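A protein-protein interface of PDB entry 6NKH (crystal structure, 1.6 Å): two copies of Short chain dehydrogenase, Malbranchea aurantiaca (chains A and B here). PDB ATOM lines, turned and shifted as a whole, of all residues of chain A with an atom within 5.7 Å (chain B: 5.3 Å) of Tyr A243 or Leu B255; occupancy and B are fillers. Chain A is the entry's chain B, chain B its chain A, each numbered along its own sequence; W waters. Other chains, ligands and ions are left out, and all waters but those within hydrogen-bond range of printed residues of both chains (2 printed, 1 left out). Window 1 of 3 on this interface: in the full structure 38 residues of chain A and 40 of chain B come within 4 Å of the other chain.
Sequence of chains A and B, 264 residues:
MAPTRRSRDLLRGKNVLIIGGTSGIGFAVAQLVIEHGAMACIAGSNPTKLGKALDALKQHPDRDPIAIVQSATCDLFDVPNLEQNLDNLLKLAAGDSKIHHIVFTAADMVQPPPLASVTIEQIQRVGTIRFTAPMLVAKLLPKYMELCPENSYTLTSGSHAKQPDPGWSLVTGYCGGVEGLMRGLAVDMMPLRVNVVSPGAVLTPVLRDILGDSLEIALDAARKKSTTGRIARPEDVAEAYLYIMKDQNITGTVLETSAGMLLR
OD2 of Asp A247 is in hydrogen-bond range of OG1 of Thr B257, 2.6 Å away. OG1 of Thr A253 lies within hydrogen-bond range of OE1 of Glu B256 (3.2 Å). OD1 of Asp A247 lies close to O of Asp B236 (3.3 Å).
The backbone carbonyl oxygen (O) of Leu B255 sits at hydrogen-bond distance from the backbone NH (N) of Ser B198 (2.7 Å). OD2 of Asp A247 is in hydrogen-bond range of OH of Tyr A243 (2.7 Å). The backbone carbonyl oxygen of Ser B198 is in hydrogen-bond range of the backbone NH of Thr B257, 3.2 Å away. The backbone carbonyl oxygen (O) of Val B196 is in hydrogen-bond range of the backbone NH (N) of Leu B255.
Among the printed residues, merely in contact across the chains: Leu A255 with Tyr B243 (3.2 Å), Ala A240 with Tyr B243 (3.3 Å), Tyr A243 with Ala B240 (3.3 Å), Ile A250 with Glu B256 (3.4 Å), Glu A239 with Tyr B243 (3.5 Å), Lys A246 with Glu B239 (3.6 Å), Tyr A243 with Glu B239 (3.7 Å), Leu A255 with Leu B255 (3.7 Å), Tyr A243 with Tyr B243 (3.7 Å), Ile A250 with Thr B257 (3.9 Å), Tyr A243 with Thr B257 (3.9 Å) and Tyr A243 with Leu B255 (3.99 Å).
Printed residues of chain B within 4 Å of Glu A239: Tyr B243. Of the printed residues of chain B, Ile A250 touches Glu B256 (3.4 Å) and Thr B257 (3.9 Å). Of the printed residues of chain B, Thr A253 touches Glu B256. Printed residues of chain B within 4 Å of Leu A255: Tyr B243 and Leu B255. The nearest printed residue of chain B that does not touch Tyr A243 is Asp B236 (4.9 Å).
Hydrophobic or aromatic side chains of chain B that line the printed part of chain A: Ala B240, Tyr B243 and Leu B255. Among the printed residues, no Asp or Glu carboxylate lies within 4 Å of a Lys or Arg side-chain nitrogen of the other chain.
Glu A239 touches Tyr B243, and with the chains exchanged Tyr A243 touches Glu B239. Ala A240 touches Tyr B243, and with the chains exchanged Tyr A243 touches Ala B240. Tyr B243 touches its own counterpart, Tyr A243. Tyr A243 touches Leu B255, and with the chains exchanged Leu A255 touches Tyr B243. Of the 15 pairs that touch across the chains among the printed residues, 8 have their exchanged pair printed and touching as well.
Water W2 bridges OE1 of Glu B239 (2.6 Å) and NZ of Lys A246 (3.3 Å). Water W1 lies within hydrogen-bond range of the side-chain hydroxyl (OG1) of Thr A253, the backbone NH (N) of Glu B256 and the backbone carbonyl oxygen (O) of Val B254.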
ATOM      1  N   ALA A 238       9.078  -9.987   5.737  1.00  0.00           N
ATOM      2  CA  ALA A 238       8.793 -11.415   5.701  1.00  0.00           C
ATOM      3  C   ALA A 238       9.908 -12.186   5.010  1.00  0.00           C
ATOM      4  O   ALA A 238      10.182 -13.330   5.376  1.00  0.00           O
ATOM      5  CB  ALA A 238       7.457 -11.672   5.009  1.00  0.00           C
ATOM      6  N   GLU A 239      10.574 -11.574   4.030  1.00  0.00           N
ATOM      7  CA  GLU A 239      11.657 -12.256   3.336  1.00  0.00           C
ATOM      8  C   GLU A 239      12.798 -12.635   4.277  1.00  0.00           C
ATOM      9  O   GLU A 239      13.572 -13.547   3.961  1.00  0.00           O
ATOM     10  CB  GLU A 239      12.196 -11.378   2.204  1.00  0.00           C
ATOM     11  CG  GLU A 239      11.239 -11.115   1.010  1.00  0.00           C
ATOM     12  CD  GLU A 239      11.023 -12.304   0.071  1.00  0.00           C
ATOM     13  OE1 GLU A 239      11.902 -13.191  -0.011  1.00  0.00           O
ATOM     14  OE2 GLU A 239       9.991 -12.316  -0.636  1.00  0.00           O
ATOM     15  N   ALA A 240      12.927 -11.955   5.419  1.00  0.00           N
ATOM     16  CA  ALA A 240      13.988 -12.268   6.372  1.00  0.00           C
ATOM     17  C   ALA A 240      13.720 -13.575   7.100  1.00  0.00           C
ATOM     18  O   ALA A 240      14.639 -14.364   7.341  1.00  0.00           O
ATOM     19  CB  ALA A 240      14.131 -11.137   7.386  1.00  0.00           C
ATOM     20  N   TYR A 241      12.470 -13.794   7.499  1.00  0.00           N
ATOM     21  CA  TYR A 241      12.099 -15.054   8.130  1.00  0.00           C
ATOM     22  C   TYR A 241      12.289 -16.221   7.173  1.00  0.00           C
ATOM     23  O   TYR A 241      12.806 -17.272   7.562  1.00  0.00           O
ATOM     24  CB  TYR A 241      10.654 -14.965   8.597  1.00  0.00           C
ATOM     25  CG  TYR A 241      10.434 -13.958   9.692  1.00  0.00           C
ATOM     26  CD1 TYR A 241      10.548 -14.313  11.022  1.00  0.00           C
ATOM     27  CD2 TYR A 241      10.136 -12.636   9.390  1.00  0.00           C
ATOM     28  CE1 TYR A 241      10.340 -13.392  12.026  1.00  0.00           C
ATOM     29  CE2 TYR A 241       9.925 -11.712  10.379  1.00  0.00           C
ATOM     30  CZ  TYR A 241      10.032 -12.090  11.694  1.00  0.00           C
ATOM     31  OH  TYR A 241       9.828 -11.173  12.688  1.00  0.00           O
ATOM     32  N   LEU A 242      11.870 -16.048   5.921  1.00  0.00           N
ATOM     33  CA  LEU A 242      12.015 -17.092   4.913  1.00  0.00           C
ATOM     34  C   LEU A 242      13.487 -17.405   4.657  1.00  0.00           C
ATOM     35  O   LEU A 242      13.871 -18.576   4.553  1.00  0.00           O
ATOM     36  CB  LEU A 242      11.330 -16.647   3.614  1.00  0.00           C
ATOM     37  CG  LEU A 242      11.196 -17.664   2.474  1.00  0.00           C
ATOM     38  CD1 LEU A 242      10.105 -18.681   2.807  1.00  0.00           C
ATOM     39  CD2 LEU A 242      10.960 -16.998   1.117  1.00  0.00           C
ATOM     40  N   TYR A 243      14.317 -16.362   4.522  1.00  0.00           N
ATOM     41  CA  TYR A 243      15.758 -16.547   4.374  1.00  0.00           C
ATOM     42  C   TYR A 243      16.342 -17.408   5.494  1.00  0.00           C
ATOM     43  O   TYR A 243      17.116 -18.333   5.240  1.00  0.00           O
ATOM     44  CB  TYR A 243      16.458 -15.181   4.316  1.00  0.00           C
ATOM     45  CG  TYR A 243      17.899 -15.271   4.758  1.00  0.00           C
ATOM     46  CD1 TYR A 243      18.832 -15.979   4.018  1.00  0.00           C
ATOM     47  CD2 TYR A 243      18.316 -14.667   5.934  1.00  0.00           C
ATOM     48  CE1 TYR A 243      20.130 -16.092   4.445  1.00  0.00           C
ATOM     49  CE2 TYR A 243      19.613 -14.771   6.362  1.00  0.00           C
ATOM     50  CZ  TYR A 243      20.518 -15.483   5.615  1.00  0.00           C
ATOM     51  OH  TYR A 243      21.813 -15.596   6.046  1.00  0.00           O
ATOM     52  N   ILE A 244      15.983 -17.115   6.743  1.00  0.00           N
ATOM     53  CA  ILE A 244      16.532 -17.869   7.866  1.00  0.00           C
ATOM     54  C   ILE A 244      16.167 -19.346   7.754  1.00  0.00           C
ATOM     55  O   ILE A 244      16.972 -20.225   8.086  1.00  0.00           O
ATOM     56  CB  ILE A 244      16.063 -17.257   9.200  1.00  0.00           C
ATOM     57  CG1 ILE A 244      16.729 -15.891   9.406  1.00  0.00           C
ATOM     58  CG2 ILE A 244      16.358 -18.200  10.362  1.00  0.00           C
ATOM     59  CD1 ILE A 244      16.189 -15.101  10.561  1.00  0.00           C
ATOM     60  N   MET A 245      14.956 -19.646   7.281  1.00  0.00           N
ATOM     61  CA  MET A 245      14.562 -21.035   7.061  1.00  0.00           C
ATOM     62  C   MET A 245      15.463 -21.712   6.039  1.00  0.00           C
ATOM     63  O   MET A 245      15.719 -22.917   6.143  1.00  0.00           O
ATOM     64  CB  MET A 245      13.111 -21.093   6.589  1.00  0.00           C
ATOM     65  CG  MET A 245      12.110 -20.565   7.598  1.00  0.00           C
ATOM     66  SD  MET A 245      10.436 -20.533   6.926  1.00  0.00           S
ATOM     67  CE  MET A 245       9.555 -19.718   8.250  1.00  0.00           C
ATOM     68  N   LYS A 246      15.957 -20.961   5.056  1.00  0.00           N
ATOM     69  CA  LYS A 246      16.700 -21.540   3.947  1.00  0.00           C
ATOM     70  C   LYS A 246      18.182 -21.719   4.254  1.00  0.00           C
ATOM     71  O   LYS A 246      18.778 -22.733   3.862  1.00  0.00           O
ATOM     72  CB  LYS A 246      16.553 -20.660   2.708  1.00  0.00           C
ATOM     73  CG  LYS A 246      15.178 -20.640   2.074  1.00  0.00           C
ATOM     74  CD  LYS A 246      15.179 -19.670   0.906  1.00  0.00           C
ATOM     75  CE  LYS A 246      13.811 -19.527   0.284  1.00  0.00           C
ATOM     76  NZ  LYS A 246      13.813 -18.518  -0.817  1.00  0.00           N
ATOM     77  N   ASP A 247      18.793 -20.756   4.946  1.00  0.00           N
ATOM     78  CA  ASP A 247      20.233 -20.755   5.215  1.00  0.00           C
ATOM     79  C   ASP A 247      20.511 -21.626   6.428  1.00  0.00           C
ATOM     80  O   ASP A 247      20.385 -21.188   7.571  1.00  0.00           O
ATOM     81  CB  ASP A 247      20.734 -19.329   5.438  1.00  0.00           C
ATOM     82  CG  ASP A 247      22.242 -19.250   5.645  1.00  0.00           C
ATOM     83  OD1 ASP A 247      22.902 -20.302   5.649  1.00  0.00           O
ATOM     84  OD2 ASP A 247      22.772 -18.131   5.817  1.00  0.00           O
ATOM     85  N   ILE A 250      22.916 -20.160   9.440  1.00  0.00           N
ATOM     86  CA  ILE A 250      22.709 -18.949  10.230  1.00  0.00           C
ATOM     87  C   ILE A 250      22.055 -19.310  11.557  1.00  0.00           C
ATOM     88  O   ILE A 250      20.953 -19.870  11.591  1.00  0.00           O
ATOM     89  CB  ILE A 250      21.881 -17.904   9.457  1.00  0.00           C
ATOM     90  CG1 ILE A 250      21.858 -16.587  10.229  1.00  0.00           C
ATOM     91  CG2 ILE A 250      20.446 -18.361   9.187  1.00  0.00           C
ATOM     92  CD1 ILE A 250      21.362 -15.429   9.426  1.00  0.00           C
ATOM     93  N   THR A 253      22.059 -15.075  15.725  1.00  0.00           N
ATOM     94  CA  THR A 253      22.232 -13.676  15.375  1.00  0.00           C
ATOM     95  C   THR A 253      20.906 -12.933  15.306  1.00  0.00           C
ATOM     96  O   THR A 253      19.825 -13.524  15.224  1.00  0.00           O
ATOM     97  CB  THR A 253      22.963 -13.517  14.041  1.00  0.00           C
ATOM     98  OG1 THR A 253      23.309 -12.132  13.857  1.00  0.00           O
ATOM     99  CG2 THR A 253      22.091 -13.983  12.913  1.00  0.00           C
ATOM    100  N   LEU A 255      18.977 -10.355  13.011  1.00  0.00           N
ATOM    101  CA  LEU A 255      18.901  -9.856  11.644  1.00  0.00           C
ATOM    102  C   LEU A 255      18.114  -8.547  11.655  1.00  0.00           C
ATOM    103  O   LEU A 255      16.923  -8.540  11.972  1.00  0.00           O
ATOM    104  CB  LEU A 255      18.231 -10.891  10.743  1.00  0.00           C
ATOM    105  CG  LEU A 255      18.274 -10.676   9.230  1.00  0.00           C
ATOM    106  CD1 LEU A 255      18.016 -11.978   8.491  1.00  0.00           C
ATOM    107  CD2 LEU A 255      17.276  -9.639   8.798  1.00  0.00           C
ATOM    108  N   VAL B 196      26.549  -5.658   4.524  1.00  0.00           N
ATOM    109  CA  VAL B 196      27.676  -6.588   4.568  1.00  0.00           C
ATOM    110  C   VAL B 196      27.162  -7.971   4.927  1.00  0.00           C
ATOM    111  O   VAL B 196      26.303  -8.111   5.804  1.00  0.00           O
ATOM    112  CB  VAL B 196      28.750  -6.154   5.582  1.00  0.00           C
ATOM    113  CG1 VAL B 196      29.741  -7.282   5.817  1.00  0.00           C
ATOM    114  CG2 VAL B 196      29.475  -4.933   5.083  1.00  0.00           C
ATOM    115  N   VAL B 197      27.674  -8.988   4.238  1.00  0.00           N
ATOM    116  CA  VAL B 197      27.532 -10.376   4.658  1.00  0.00           C
ATOM    117  C   VAL B 197      28.833 -10.792   5.322  1.00  0.00           C
ATOM    118  O   VAL B 197      29.918 -10.531   4.793  1.00  0.00           O
ATOM    119  CB  VAL B 197      27.191 -11.298   3.481  1.00  0.00           C
ATOM    120  CG1 VAL B 197      27.268 -12.758   3.916  1.00  0.00           C
ATOM    121  CG2 VAL B 197      25.794 -10.986   2.946  1.00  0.00           C
ATOM    122  N   SER B 198      28.723 -11.428   6.488  1.00  0.00           N
ATOM    123  CA  SER B 198      29.878 -11.835   7.282  1.00  0.00           C
ATOM    124  C   SER B 198      29.825 -13.350   7.427  1.00  0.00           C
ATOM    125  O   SER B 198      29.185 -13.873   8.349  1.00  0.00           O
ATOM    126  CB  SER B 198      29.887 -11.141   8.637  1.00  0.00           C
ATOM    127  OG  SER B 198      31.031 -11.501   9.381  1.00  0.00           O
ATOM    128  N   PRO B 199      30.460 -14.091   6.526  1.00  0.00           N
ATOM    129  CA  PRO B 199      30.401 -15.554   6.589  1.00  0.00           C
ATOM    130  C   PRO B 199      31.436 -16.148   7.531  1.00  0.00           C
ATOM    131  O   PRO B 199      32.457 -15.536   7.855  1.00  0.00           O
ATOM    132  CB  PRO B 199      30.673 -15.977   5.139  1.00  0.00           C
ATOM    133  CG  PRO B 199      31.497 -14.889   4.584  1.00  0.00           C
ATOM    134  CD  PRO B 199      31.036 -13.622   5.254  1.00  0.00           C
ATOM    135  N   ASP B 236      24.530 -22.235   1.057  1.00  0.00           N
ATOM    136  CA  ASP B 236      23.881 -21.673   2.240  1.00  0.00           C
ATOM    137  C   ASP B 236      24.156 -20.181   2.349  1.00  0.00           C
ATOM    138  O   ASP B 236      23.237 -19.375   2.538  1.00  0.00           O
ATOM    139  CB  ASP B 236      24.373 -22.385   3.506  1.00  0.00           C
ATOM    140  CG  ASP B 236      23.793 -23.779   3.679  1.00  0.00           C
ATOM    141  OD1 ASP B 236      22.610 -23.998   3.334  1.00  0.00           O
ATOM    142  OD2 ASP B 236      24.535 -24.664   4.160  1.00  0.00           O
ATOM    143  N   GLU B 239      22.453 -17.649  -0.148  1.00  0.00           N
ATOM    144  CA  GLU B 239      21.085 -17.220   0.118  1.00  0.00           C
ATOM    145  C   GLU B 239      21.050 -15.870   0.827  1.00  0.00           C
ATOM    146  O   GLU B 239      20.094 -15.110   0.654  1.00  0.00           O
ATOM    147  CB  GLU B 239      20.340 -18.262   0.963  1.00  0.00           C
ATOM    148  CG  GLU B 239      20.011 -19.589   0.286  1.00  0.00           C
ATOM    149  CD  GLU B 239      18.964 -19.492  -0.814  1.00  0.00           C
ATOM    150  OE1 GLU B 239      18.159 -18.539  -0.819  1.00  0.00           O
ATOM    151  OE2 GLU B 239      18.915 -20.412  -1.658  1.00  0.00           O
ATOM    152  N   ALA B 240      22.078 -15.551   1.620  1.00  0.00           N
ATOM    153  CA  ALA B 240      22.095 -14.288   2.348  1.00  0.00           C
ATOM    154  C   ALA B 240      22.199 -13.093   1.405  1.00  0.00           C
ATOM    155  O   ALA B 240      21.529 -12.076   1.611  1.00  0.00           O
ATOM    156  CB  ALA B 240      23.249 -14.274   3.344  1.00  0.00           C
ATOM    157  N   TYR B 243      18.741 -12.783  -0.285  1.00  0.00           N
ATOM    158  CA  TYR B 243      17.831 -12.129   0.647  1.00  0.00           C
ATOM    159  C   TYR B 243      17.981 -10.611   0.611  1.00  0.00           C
ATOM    160  O   TYR B 243      16.990  -9.875   0.532  1.00  0.00           O
ATOM    161  CB  TYR B 243      18.068 -12.654   2.062  1.00  0.00           C
ATOM    162  CG  TYR B 243      17.554 -11.689   3.088  1.00  0.00           C
ATOM    163  CD1 TYR B 243      16.201 -11.431   3.215  1.00  0.00           C
ATOM    164  CD2 TYR B 243      18.432 -11.011   3.918  1.00  0.00           C
ATOM    165  CE1 TYR B 243      15.736 -10.519   4.143  1.00  0.00           C
ATOM    166  CE2 TYR B 243      17.981 -10.108   4.844  1.00  0.00           C
ATOM    167  CZ  TYR B 243      16.632  -9.862   4.954  1.00  0.00           C
ATOM    168  OH  TYR B 243      16.189  -8.948   5.878  1.00  0.00           O
ATOM    169  N   ILE B 244      19.219 -10.126   0.679  1.00  0.00           N
ATOM    170  CA  ILE B 244      19.463  -8.686   0.714  1.00  0.00           C
ATOM    171  C   ILE B 244      18.928  -8.018  -0.546  1.00  0.00           C
ATOM    172  O   ILE B 244      18.427  -6.887  -0.500  1.00  0.00           O
ATOM    173  CB  ILE B 244      20.966  -8.418   0.923  1.00  0.00           C
ATOM    174  CG1 ILE B 244      21.365  -8.831   2.347  1.00  0.00           C
ATOM    175  CG2 ILE B 244      21.303  -6.969   0.641  1.00  0.00           C
ATOM    176  CD1 ILE B 244      22.853  -8.837   2.602  1.00  0.00           C
ATOM    177  N   THR B 253      23.461  -2.883   7.726  1.00  0.00           N
ATOM    178  CA  THR B 253      23.694  -3.916   8.720  1.00  0.00           C
ATOM    179  C   THR B 253      24.681  -4.968   8.231  1.00  0.00           C
ATOM    180  O   THR B 253      24.985  -5.087   7.040  1.00  0.00           O
ATOM    181  CB  THR B 253      22.372  -4.576   9.145  1.00  0.00           C
ATOM    182  OG1 THR B 253      22.611  -5.454  10.260  1.00  0.00           O
ATOM    183  CG2 THR B 253      21.761  -5.343   8.013  1.00  0.00           C
ATOM    184  N   VAL B 254      25.204  -5.704   9.201  1.00  0.00           N
ATOM    185  CA  VAL B 254      26.145  -6.787   8.978  1.00  0.00           C
ATOM    186  C   VAL B 254      25.384  -8.074   9.244  1.00  0.00           C
ATOM    187  O   VAL B 254      24.998  -8.353  10.387  1.00  0.00           O
ATOM    188  CB  VAL B 254      27.378  -6.665   9.884  1.00  0.00           C
ATOM    189  CG1 VAL B 254      28.289  -7.867   9.709  1.00  0.00           C
ATOM    190  CG2 VAL B 254      28.126  -5.376   9.601  1.00  0.00           C
ATOM    191  N   LEU B 255      25.144  -8.847   8.191  1.00  0.00           N
ATOM    192  CA  LEU B 255      24.414 -10.103   8.292  1.00  0.00           C
ATOM    193  C   LEU B 255      25.408 -11.233   8.543  1.00  0.00           C
ATOM    194  O   LEU B 255      26.286 -11.487   7.716  1.00  0.00           O
ATOM    195  CB  LEU B 255      23.601 -10.346   7.025  1.00  0.00           C
ATOM    196  CG  LEU B 255      22.706 -11.580   6.975  1.00  0.00           C
ATOM    197  CD1 LEU B 255      21.715 -11.554   8.119  1.00  0.00           C
ATOM    198  CD2 LEU B 255      21.970 -11.625   5.650  1.00  0.00           C
ATOM    199  N   GLU B 256      25.253 -11.906   9.680  1.00  0.00           N
ATOM    200  CA  GLU B 256      26.206 -12.898  10.174  1.00  0.00           C
ATOM    201  C   GLU B 256      25.656 -14.297   9.910  1.00  0.00           C
ATOM    202  O   GLU B 256      24.657 -14.702  10.511  1.00  0.00           O
ATOM    203  CB  GLU B 256      26.449 -12.678  11.667  1.00  0.00           C
ATOM    204  CG  GLU B 256      27.158 -11.377  11.976  1.00  0.00           C
ATOM    205  CD  GLU B 256      27.205 -11.048  13.449  1.00  0.00           C
ATOM    206  OE1 GLU B 256      26.439 -11.649  14.239  1.00  0.00           O
ATOM    207  OE2 GLU B 256      28.038 -10.197  13.822  1.00  0.00           O
ATOM    208  N   THR B 257      26.309 -15.033   9.020  1.00  0.00           N
ATOM    209  CA  THR B 257      25.970 -16.423   8.731  1.00  0.00           C
ATOM    210  C   THR B 257      27.244 -17.248   8.945  1.00  0.00           C
ATOM    211  O   THR B 257      28.042 -17.454   8.029  1.00  0.00           O
ATOM    212  CB  THR B 257      25.375 -16.561   7.333  1.00  0.00           C
ATOM    213  OG1 THR B 257      25.089 -17.939   7.086  1.00  0.00           O
ATOM    214  CG2 THR B 257      26.272 -15.973   6.254  1.00  0.00           C
HETATM  215  O   HOH W   1      23.173 -10.670  11.363  1.00  0.00           O
HETATM  216  O   HOH W   2      16.479 -18.476  -2.810  1.00  0.00           O
